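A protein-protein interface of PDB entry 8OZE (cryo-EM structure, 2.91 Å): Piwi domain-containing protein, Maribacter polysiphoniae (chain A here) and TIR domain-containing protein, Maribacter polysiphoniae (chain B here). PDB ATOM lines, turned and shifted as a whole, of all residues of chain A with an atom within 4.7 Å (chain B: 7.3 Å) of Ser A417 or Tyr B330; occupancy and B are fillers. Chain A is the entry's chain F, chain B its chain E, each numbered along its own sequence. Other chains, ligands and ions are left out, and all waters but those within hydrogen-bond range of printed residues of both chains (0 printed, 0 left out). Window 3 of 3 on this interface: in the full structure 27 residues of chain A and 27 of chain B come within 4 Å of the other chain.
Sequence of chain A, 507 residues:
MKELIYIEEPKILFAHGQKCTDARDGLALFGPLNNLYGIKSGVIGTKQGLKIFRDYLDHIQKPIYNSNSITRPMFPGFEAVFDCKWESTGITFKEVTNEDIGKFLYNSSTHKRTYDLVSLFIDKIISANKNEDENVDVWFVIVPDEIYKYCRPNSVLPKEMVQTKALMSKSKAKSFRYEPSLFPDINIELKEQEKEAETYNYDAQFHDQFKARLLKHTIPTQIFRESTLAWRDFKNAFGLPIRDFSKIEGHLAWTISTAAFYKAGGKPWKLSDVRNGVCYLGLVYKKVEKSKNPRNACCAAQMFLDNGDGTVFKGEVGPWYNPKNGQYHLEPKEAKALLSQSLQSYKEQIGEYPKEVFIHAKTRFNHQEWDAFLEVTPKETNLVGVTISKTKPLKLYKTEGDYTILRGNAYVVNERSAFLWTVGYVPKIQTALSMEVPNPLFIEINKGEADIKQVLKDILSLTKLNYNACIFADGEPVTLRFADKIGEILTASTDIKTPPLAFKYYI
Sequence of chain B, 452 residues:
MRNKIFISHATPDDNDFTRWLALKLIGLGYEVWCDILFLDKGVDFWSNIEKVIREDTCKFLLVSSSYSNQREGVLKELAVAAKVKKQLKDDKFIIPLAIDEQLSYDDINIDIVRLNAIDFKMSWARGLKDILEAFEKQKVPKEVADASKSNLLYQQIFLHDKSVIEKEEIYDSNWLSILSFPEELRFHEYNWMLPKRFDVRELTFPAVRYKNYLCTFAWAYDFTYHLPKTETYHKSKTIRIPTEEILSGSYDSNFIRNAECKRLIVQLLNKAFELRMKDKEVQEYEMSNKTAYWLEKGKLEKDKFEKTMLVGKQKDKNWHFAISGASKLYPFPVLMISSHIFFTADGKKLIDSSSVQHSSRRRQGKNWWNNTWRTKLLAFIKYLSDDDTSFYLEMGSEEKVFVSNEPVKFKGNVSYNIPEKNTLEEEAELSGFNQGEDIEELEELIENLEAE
OD1 of Asn A414 sits at hydrogen-bond distance from OH of Tyr B330. The side-chain hydroxyl of Tyr B330 sits at hydrogen-bond distance from the side-chain hydroxyl of Ser A417, 2.9 Å away.
Of the printed residues of chain B, Asn A414 touches Tyr B330 (3.5 Å). Of chain B, only Tyr B330 comes within 4 Å of Ser A417. Tyr B330 touches three residues of chain A. Printed residues of chain A within 4 Å of Phe B332: Tyr A411 (3.0 Å).
Among the printed residues, pairs that only touch across the chains: Tyr A411 with Phe B332 (3.0 Å) and Phe A442 with Tyr B330 (3.9 Å).
Of the 13 printed residues of chain A, 4 touch a printed residue of chain B. Hydrophobic or aromatic side chains of chain A within 4 Å of the printed part of chain B: Tyr A411 and Phe A442. Of the 12 printed residues of chain B, 2 touch a printed residue of chain A. Hydrophobic or aromatic side chains of chain B that line the printed part of chain A: Tyr B330 and Phe B332. Among the printed residues, 4 pairs touch across the chains. Among the printed residues, no Asp or Glu carboxylate lies within 4 Å of a Lys or Arg side-chain nitrogen of the other chain.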
ATOM      1  N   TYR A 411      27.969   1.266   8.067  1.00  0.00           N
ATOM      2  CA  TYR A 411      27.621   2.606   8.524  1.00  0.00           C
ATOM      3  C   TYR A 411      26.122   2.789   8.336  1.00  0.00           C
ATOM      4  O   TYR A 411      25.654   3.024   7.218  1.00  0.00           O
ATOM      5  CB  TYR A 411      28.404   3.667   7.757  1.00  0.00           C
ATOM      6  CG  TYR A 411      27.916   5.072   8.013  1.00  0.00           C
ATOM      7  CD1 TYR A 411      27.592   5.493   9.295  1.00  0.00           C
ATOM      8  CD2 TYR A 411      27.762   5.973   6.972  1.00  0.00           C
ATOM      9  CE1 TYR A 411      27.136   6.768   9.533  1.00  0.00           C
ATOM     10  CE2 TYR A 411      27.307   7.253   7.202  1.00  0.00           C
ATOM     11  CZ  TYR A 411      26.996   7.643   8.485  1.00  0.00           C
ATOM     12  OH  TYR A 411      26.543   8.916   8.722  1.00  0.00           O
ATOM     13  N   VAL A 412      25.367   2.682   9.427  1.00  0.00           N
ATOM     14  CA  VAL A 412      23.917   2.841   9.376  1.00  0.00           C
ATOM     15  C   VAL A 412      23.632   4.336   9.268  1.00  0.00           C
ATOM     16  O   VAL A 412      23.707   5.067  10.257  1.00  0.00           O
ATOM     17  CB  VAL A 412      23.229   2.216  10.590  1.00  0.00           C
ATOM     18  CG1 VAL A 412      21.748   2.543  10.581  1.00  0.00           C
ATOM     19  CG2 VAL A 412      23.434   0.718  10.591  1.00  0.00           C
ATOM     20  N   VAL A 413      23.317   4.797   8.057  1.00  0.00           N
ATOM     21  CA  VAL A 413      23.022   6.211   7.851  1.00  0.00           C
ATOM     22  C   VAL A 413      21.794   6.613   8.654  1.00  0.00           C
ATOM     23  O   VAL A 413      21.784   7.642   9.338  1.00  0.00           O
ATOM     24  CB  VAL A 413      22.841   6.510   6.353  1.00  0.00           C
ATOM     25  CG1 VAL A 413      22.372   7.938   6.151  1.00  0.00           C
ATOM     26  CG2 VAL A 413      24.139   6.262   5.606  1.00  0.00           C
ATOM     27  N   ASN A 414      20.744   5.800   8.591  1.00  0.00           N
ATOM     28  CA  ASN A 414      19.553   6.002   9.406  1.00  0.00           C
ATOM     29  C   ASN A 414      18.753   4.708   9.398  1.00  0.00           C
ATOM     30  O   ASN A 414      19.102   3.744   8.710  1.00  0.00           O
ATOM     31  CB  ASN A 414      18.719   7.183   8.903  1.00  0.00           C
ATOM     32  CG  ASN A 414      18.453   7.117   7.419  1.00  0.00           C
ATOM     33  OD1 ASN A 414      19.321   6.736   6.638  1.00  0.00           O
ATOM     34  ND2 ASN A 414      17.246   7.490   7.018  1.00  0.00           N
ATOM     35  N   GLU A 415      17.649   4.706  10.149  1.00  0.00           N
ATOM     36  CA  GLU A 415      16.828   3.510  10.313  1.00  0.00           C
ATOM     37  C   GLU A 415      16.334   2.934   8.992  1.00  0.00           C
ATOM     38  O   GLU A 415      15.766   1.838   8.992  1.00  0.00           O
ATOM     39  CB  GLU A 415      15.630   3.819  11.211  1.00  0.00           C
ATOM     40  CG  GLU A 415      14.705   4.890  10.659  1.00  0.00           C
ATOM     41  CD  GLU A 415      13.346   4.894  11.330  1.00  0.00           C
ATOM     42  OE1 GLU A 415      13.231   4.354  12.450  1.00  0.00           O
ATOM     43  OE2 GLU A 415      12.390   5.436  10.736  1.00  0.00           O
ATOM     44  N   ARG A 416      16.526   3.637   7.877  1.00  0.00           N
ATOM     45  CA  ARG A 416      16.104   3.151   6.574  1.00  0.00           C
ATOM     46  C   ARG A 416      17.227   2.995   5.561  1.00  0.00           C
ATOM     47  O   ARG A 416      16.971   2.466   4.475  1.00  0.00           O
ATOM     48  CB  ARG A 416      15.037   4.080   5.975  1.00  0.00           C
ATOM     49  CG  ARG A 416      13.765   4.163   6.787  1.00  0.00           C
ATOM     50  CD  ARG A 416      12.668   4.855   6.002  1.00  0.00           C
ATOM     51  NE  ARG A 416      12.012   3.956   5.058  1.00  0.00           N
ATOM     52  CZ  ARG A 416      11.210   2.956   5.398  1.00  0.00           C
ATOM     53  NH1 ARG A 416      10.930   2.691   6.664  1.00  0.00           N
ATOM     54  NH2 ARG A 416      10.674   2.203   4.444  1.00  0.00           N
ATOM     55  N   SER A 417      18.448   3.434   5.865  1.00  0.00           N
ATOM     56  CA  SER A 417      19.526   3.362   4.890  1.00  0.00           C
ATOM     57  C   SER A 417      20.849   3.103   5.589  1.00  0.00           C
ATOM     58  O   SER A 417      21.085   3.584   6.699  1.00  0.00           O
ATOM     59  CB  SER A 417      19.631   4.645   4.064  1.00  0.00           C
ATOM     60  OG  SER A 417      18.504   4.806   3.222  1.00  0.00           O
ATOM     61  N   ALA A 418      21.721   2.361   4.907  1.00  0.00           N
ATOM     62  CA  ALA A 418      23.019   2.013   5.461  1.00  0.00           C
ATOM     63  C   ALA A 418      23.980   1.673   4.334  1.00  0.00           C
ATOM     64  O   ALA A 418      23.578   1.422   3.195  1.00  0.00           O
ATOM     65  CB  ALA A 418      22.913   0.839   6.438  1.00  0.00           C
ATOM     66  N   PHE A 442      25.240  -0.061  -0.967  1.00  0.00           N
ATOM     67  CA  PHE A 442      24.283   0.879  -0.390  1.00  0.00           C
ATOM     68  C   PHE A 442      22.943   0.172  -0.253  1.00  0.00           C
ATOM     69  O   PHE A 442      22.240  -0.047  -1.240  1.00  0.00           O
ATOM     70  CB  PHE A 442      24.160   2.130  -1.248  1.00  0.00           C
ATOM     71  CG  PHE A 442      23.271   3.177  -0.654  1.00  0.00           C
ATOM     72  CD1 PHE A 442      23.266   3.406   0.706  1.00  0.00           C
ATOM     73  CD2 PHE A 442      22.422   3.916  -1.453  1.00  0.00           C
ATOM     74  CE1 PHE A 442      22.444   4.361   1.256  1.00  0.00           C
ATOM     75  CE2 PHE A 442      21.597   4.873  -0.908  1.00  0.00           C
ATOM     76  CZ  PHE A 442      21.608   5.095   0.447  1.00  0.00           C
ATOM     77  N   ILE A 443      22.579  -0.187   0.974  1.00  0.00           N
ATOM     78  CA  ILE A 443      21.333  -0.890   1.250  1.00  0.00           C
ATOM     79  C   ILE A 443      20.316   0.111   1.772  1.00  0.00           C
ATOM     80  O   ILE A 443      20.515   0.726   2.825  1.00  0.00           O
ATOM     81  CB  ILE A 443      21.538  -2.042   2.245  1.00  0.00           C
ATOM     82  CG1 ILE A 443      22.475  -3.099   1.660  1.00  0.00           C
ATOM     83  CG2 ILE A 443      20.203  -2.639   2.649  1.00  0.00           C
ATOM     84  CD1 ILE A 443      23.926  -2.868   1.930  1.00  0.00           C
ATOM     85  N   GLU A 444      19.216   0.257   1.044  1.00  0.00           N
ATOM     86  CA  GLU A 444      18.156   1.191   1.383  1.00  0.00           C
ATOM     87  C   GLU A 444      16.847   0.427   1.464  1.00  0.00           C
ATOM     88  O   GLU A 444      16.524  -0.342   0.554  1.00  0.00           O
ATOM     89  CB  GLU A 444      18.049   2.300   0.331  1.00  0.00           C
ATOM     90  CG  GLU A 444      17.018   3.369   0.639  1.00  0.00           C
ATOM     91  CD  GLU A 444      16.985   4.465  -0.410  1.00  0.00           C
ATOM     92  OE1 GLU A 444      17.755   4.376  -1.388  1.00  0.00           O
ATOM     93  OE2 GLU A 444      16.184   5.412  -0.262  1.00  0.00           O
ATOM     94  N   ILE A 445      16.098   0.628   2.546  1.00  0.00           N
ATOM     95  CA  ILE A 445      14.741   0.099   2.603  1.00  0.00           C
ATOM     96  C   ILE A 445      13.864   1.070   1.830  1.00  0.00           C
ATOM     97  O   ILE A 445      13.338   2.038   2.392  1.00  0.00           O
ATOM     98  CB  ILE A 445      14.232  -0.088   4.045  1.00  0.00           C
ATOM     99  CG1 ILE A 445      15.066  -1.119   4.795  1.00  0.00           C
ATOM    100  CG2 ILE A 445      12.793  -0.543   4.044  1.00  0.00           C
ATOM    101  CD1 ILE A 445      16.199  -0.528   5.564  1.00  0.00           C
ATOM    102  N   ILE A 452      16.748  -2.235   9.995  1.00  0.00           N
ATOM    103  CA  ILE A 452      17.941  -2.051   9.173  1.00  0.00           C
ATOM    104  C   ILE A 452      19.027  -3.053   9.550  1.00  0.00           C
ATOM    105  O   ILE A 452      19.681  -3.634   8.675  1.00  0.00           O
ATOM    106  CB  ILE A 452      18.439  -0.597   9.269  1.00  0.00           C
ATOM    107  CG1 ILE A 452      19.684  -0.402   8.403  1.00  0.00           C
ATOM    108  CG2 ILE A 452      18.692  -0.194  10.716  1.00  0.00           C
ATOM    109  CD1 ILE A 452      19.445  -0.597   6.931  1.00  0.00           C
ATOM    110  N   TRP B 175      34.899  11.742   1.705  1.00  0.00           N
ATOM    111  CA  TRP B 175      33.884  12.784   1.784  1.00  0.00           C
ATOM    112  C   TRP B 175      34.468  13.991   2.506  1.00  0.00           C
ATOM    113  O   TRP B 175      34.943  13.865   3.639  1.00  0.00           O
ATOM    114  CB  TRP B 175      32.652  12.282   2.532  1.00  0.00           C
ATOM    115  CG  TRP B 175      31.917  11.170   1.865  1.00  0.00           C
ATOM    116  CD1 TRP B 175      32.246  10.549   0.699  1.00  0.00           C
ATOM    117  CD2 TRP B 175      30.722  10.538   2.334  1.00  0.00           C
ATOM    118  NE1 TRP B 175      31.327   9.571   0.409  1.00  0.00           N
ATOM    119  CE2 TRP B 175      30.381   9.545   1.399  1.00  0.00           C
ATOM    120  CE3 TRP B 175      29.907  10.718   3.455  1.00  0.00           C
ATOM    121  CZ2 TRP B 175      29.261   8.735   1.550  1.00  0.00           C
ATOM    122  CZ3 TRP B 175      28.797   9.915   3.602  1.00  0.00           C
ATOM    123  CH2 TRP B 175      28.482   8.936   2.655  1.00  0.00           C
ATOM    124  N   LYS B 262      17.014  21.274  -3.351  1.00  0.00           N
ATOM    125  CA  LYS B 262      18.307  20.736  -2.957  1.00  0.00           C
ATOM    126  C   LYS B 262      19.117  20.254  -4.148  1.00  0.00           C
ATOM    127  O   LYS B 262      20.351  20.256  -4.092  1.00  0.00           O
ATOM    128  CB  LYS B 262      18.119  19.589  -1.962  1.00  0.00           C
ATOM    129  CG  LYS B 262      17.505  20.021  -0.645  1.00  0.00           C
ATOM    130  CD  LYS B 262      17.578  18.924   0.403  1.00  0.00           C
ATOM    131  CE  LYS B 262      16.593  17.810   0.111  1.00  0.00           C
ATOM    132  NZ  LYS B 262      16.539  16.830   1.229  1.00  0.00           N
ATOM    133  N   VAL B 266      23.113  21.404  -5.347  1.00  0.00           N
ATOM    134  CA  VAL B 266      24.143  20.458  -5.766  1.00  0.00           C
ATOM    135  C   VAL B 266      24.746  20.880  -7.100  1.00  0.00           C
ATOM    136  O   VAL B 266      25.966  20.818  -7.293  1.00  0.00           O
ATOM    137  CB  VAL B 266      23.560  19.037  -5.827  1.00  0.00           C
ATOM    138  CG1 VAL B 266      24.474  18.127  -6.616  1.00  0.00           C
ATOM    139  CG2 VAL B 266      23.348  18.496  -4.425  1.00  0.00           C
ATOM    140  N   SER B 327      29.174  17.013  -5.397  1.00  0.00           N
ATOM    141  CA  SER B 327      28.512  17.414  -4.166  1.00  0.00           C
ATOM    142  C   SER B 327      27.234  16.615  -3.960  1.00  0.00           C
ATOM    143  O   SER B 327      26.483  16.362  -4.904  1.00  0.00           O
ATOM    144  CB  SER B 327      28.196  18.906  -4.191  1.00  0.00           C
ATOM    145  OG  SER B 327      29.323  19.664  -3.791  1.00  0.00           O
ATOM    146  N   LYS B 328      26.997  16.207  -2.716  1.00  0.00           N
ATOM    147  CA  LYS B 328      25.794  15.479  -2.344  1.00  0.00           C
ATOM    148  C   LYS B 328      25.274  16.043  -1.034  1.00  0.00           C
ATOM    149  O   LYS B 328      26.041  16.595  -0.243  1.00  0.00           O
ATOM    150  CB  LYS B 328      26.063  13.978  -2.202  1.00  0.00           C
ATOM    151  CG  LYS B 328      26.578  13.313  -3.465  1.00  0.00           C
ATOM    152  CD  LYS B 328      25.493  13.207  -4.515  1.00  0.00           C
ATOM    153  CE  LYS B 328      26.021  12.560  -5.776  1.00  0.00           C
ATOM    154  NZ  LYS B 328      26.368  11.134  -5.555  1.00  0.00           N
ATOM    155  N   LEU B 329      23.970  15.908  -0.809  1.00  0.00           N
ATOM    156  CA  LEU B 329      23.339  16.427   0.394  1.00  0.00           C
ATOM    157  C   LEU B 329      22.610  15.368   1.207  1.00  0.00           C
ATOM    158  O   LEU B 329      22.048  15.698   2.255  1.00  0.00           O
ATOM    159  CB  LEU B 329      22.354  17.547   0.037  1.00  0.00           C
ATOM    160  CG  LEU B 329      22.909  18.773  -0.683  1.00  0.00           C
ATOM    161  CD1 LEU B 329      21.787  19.744  -0.998  1.00  0.00           C
ATOM    162  CD2 LEU B 329      23.976  19.443   0.157  1.00  0.00           C
ATOM    163  N   TYR B 330      22.597  14.103   0.760  1.00  0.00           N
ATOM    164  CA  TYR B 330      21.723  13.127   1.413  1.00  0.00           C
ATOM    165  C   TYR B 330      22.227  12.734   2.798  1.00  0.00           C
ATOM    166  O   TYR B 330      21.529  13.008   3.790  1.00  0.00           O
ATOM    167  CB  TYR B 330      21.510  11.915   0.505  1.00  0.00           C
ATOM    168  CG  TYR B 330      20.889  10.755   1.240  1.00  0.00           C
ATOM    169  CD1 TYR B 330      19.567  10.813   1.657  1.00  0.00           C
ATOM    170  CD2 TYR B 330      21.622   9.615   1.537  1.00  0.00           C
ATOM    171  CE1 TYR B 330      18.989   9.767   2.335  1.00  0.00           C
ATOM    172  CE2 TYR B 330      21.050   8.560   2.219  1.00  0.00           C
ATOM    173  CZ  TYR B 330      19.731   8.646   2.615  1.00  0.00           C
ATOM    174  OH  TYR B 330      19.145   7.606   3.292  1.00  0.00           O
ATOM    175  N   PRO B 331      23.407  12.094   2.956  1.00  0.00           N
ATOM    176  CA  PRO B 331      23.842  11.736   4.312  1.00  0.00           C
ATOM    177  C   PRO B 331      24.180  12.978   5.117  1.00  0.00           C
ATOM    178  O   PRO B 331      23.694  13.175   6.235  1.00  0.00           O
ATOM    179  CB  PRO B 331      25.079  10.858   4.075  1.00  0.00           C
ATOM    180  CG  PRO B 331      25.145  10.630   2.593  1.00  0.00           C
ATOM    181  CD  PRO B 331      24.462  11.792   1.974  1.00  0.00           C
ATOM    182  N   PHE B 332      25.019  13.824   4.536  1.00  0.00           N
ATOM    183  CA  PHE B 332      25.366  15.137   5.055  1.00  0.00           C
ATOM    184  C   PHE B 332      25.514  16.050   3.848  1.00  0.00           C
ATOM    185  O   PHE B 332      25.494  15.565   2.711  1.00  0.00           O
ATOM    186  CB  PHE B 332      26.670  15.111   5.856  1.00  0.00           C
ATOM    187  CG  PHE B 332      26.767  13.991   6.843  1.00  0.00           C
ATOM    188  CD1 PHE B 332      27.204  12.739   6.450  1.00  0.00           C
ATOM    189  CD2 PHE B 332      26.427  14.191   8.169  1.00  0.00           C
ATOM    190  CE1 PHE B 332      27.296  11.708   7.358  1.00  0.00           C
ATOM    191  CE2 PHE B 332      26.518  13.162   9.082  1.00  0.00           C
ATOM    192  CZ  PHE B 332      26.952  11.919   8.673  1.00  0.00           C
ATOM    193  N   PRO B 333      25.653  17.357   4.029  1.00  0.00           N
ATOM    194  CA  PRO B 333      26.184  18.164   2.928  1.00  0.00           C
ATOM    195  C   PRO B 333      27.670  17.897   2.782  1.00  0.00           C
ATOM    196  O   PRO B 333      28.479  18.409   3.560  1.00  0.00           O
ATOM    197  CB  PRO B 333      25.891  19.602   3.364  1.00  0.00           C
ATOM    198  CG  PRO B 333      25.787  19.530   4.846  1.00  0.00           C
ATOM    199  CD  PRO B 333      25.192  18.189   5.152  1.00  0.00           C
ATOM    200  N   VAL B 334      28.042  17.094   1.786  1.00  0.00           N
ATOM    201  CA  VAL B 334      29.414  16.639   1.618  1.00  0.00           C
ATOM    202  C   VAL B 334      29.805  16.755   0.155  1.00  0.00           C
ATOM    203  O   VAL B 334      28.972  16.972  -0.726  1.00  0.00           O
ATOM    204  CB  VAL B 334      29.630  15.183   2.090  1.00  0.00           C
ATOM    205  CG1 VAL B 334      29.461  15.071   3.592  1.00  0.00           C
ATOM    206  CG2 VAL B 334      28.684  14.245   1.362  1.00  0.00           C
ATOM    207  N   MET B 336      31.953  14.381  -2.380  1.00  0.00           N
ATOM    208  CA  MET B 336      32.624  13.111  -2.602  1.00  0.00           C
ATOM    209  C   MET B 336      33.705  13.289  -3.655  1.00  0.00           C
ATOM    210  O   MET B 336      33.482  13.940  -4.681  1.00  0.00           O
ATOM    211  CB  MET B 336      31.625  12.049  -3.056  1.00  0.00           C
ATOM    212  CG  MET B 336      30.492  11.784  -2.085  1.00  0.00           C
ATOM    213  SD  MET B 336      29.153  10.868  -2.869  1.00  0.00           S
ATOM    214  CE  MET B 336      28.220  10.331  -1.441  1.00  0.00           C
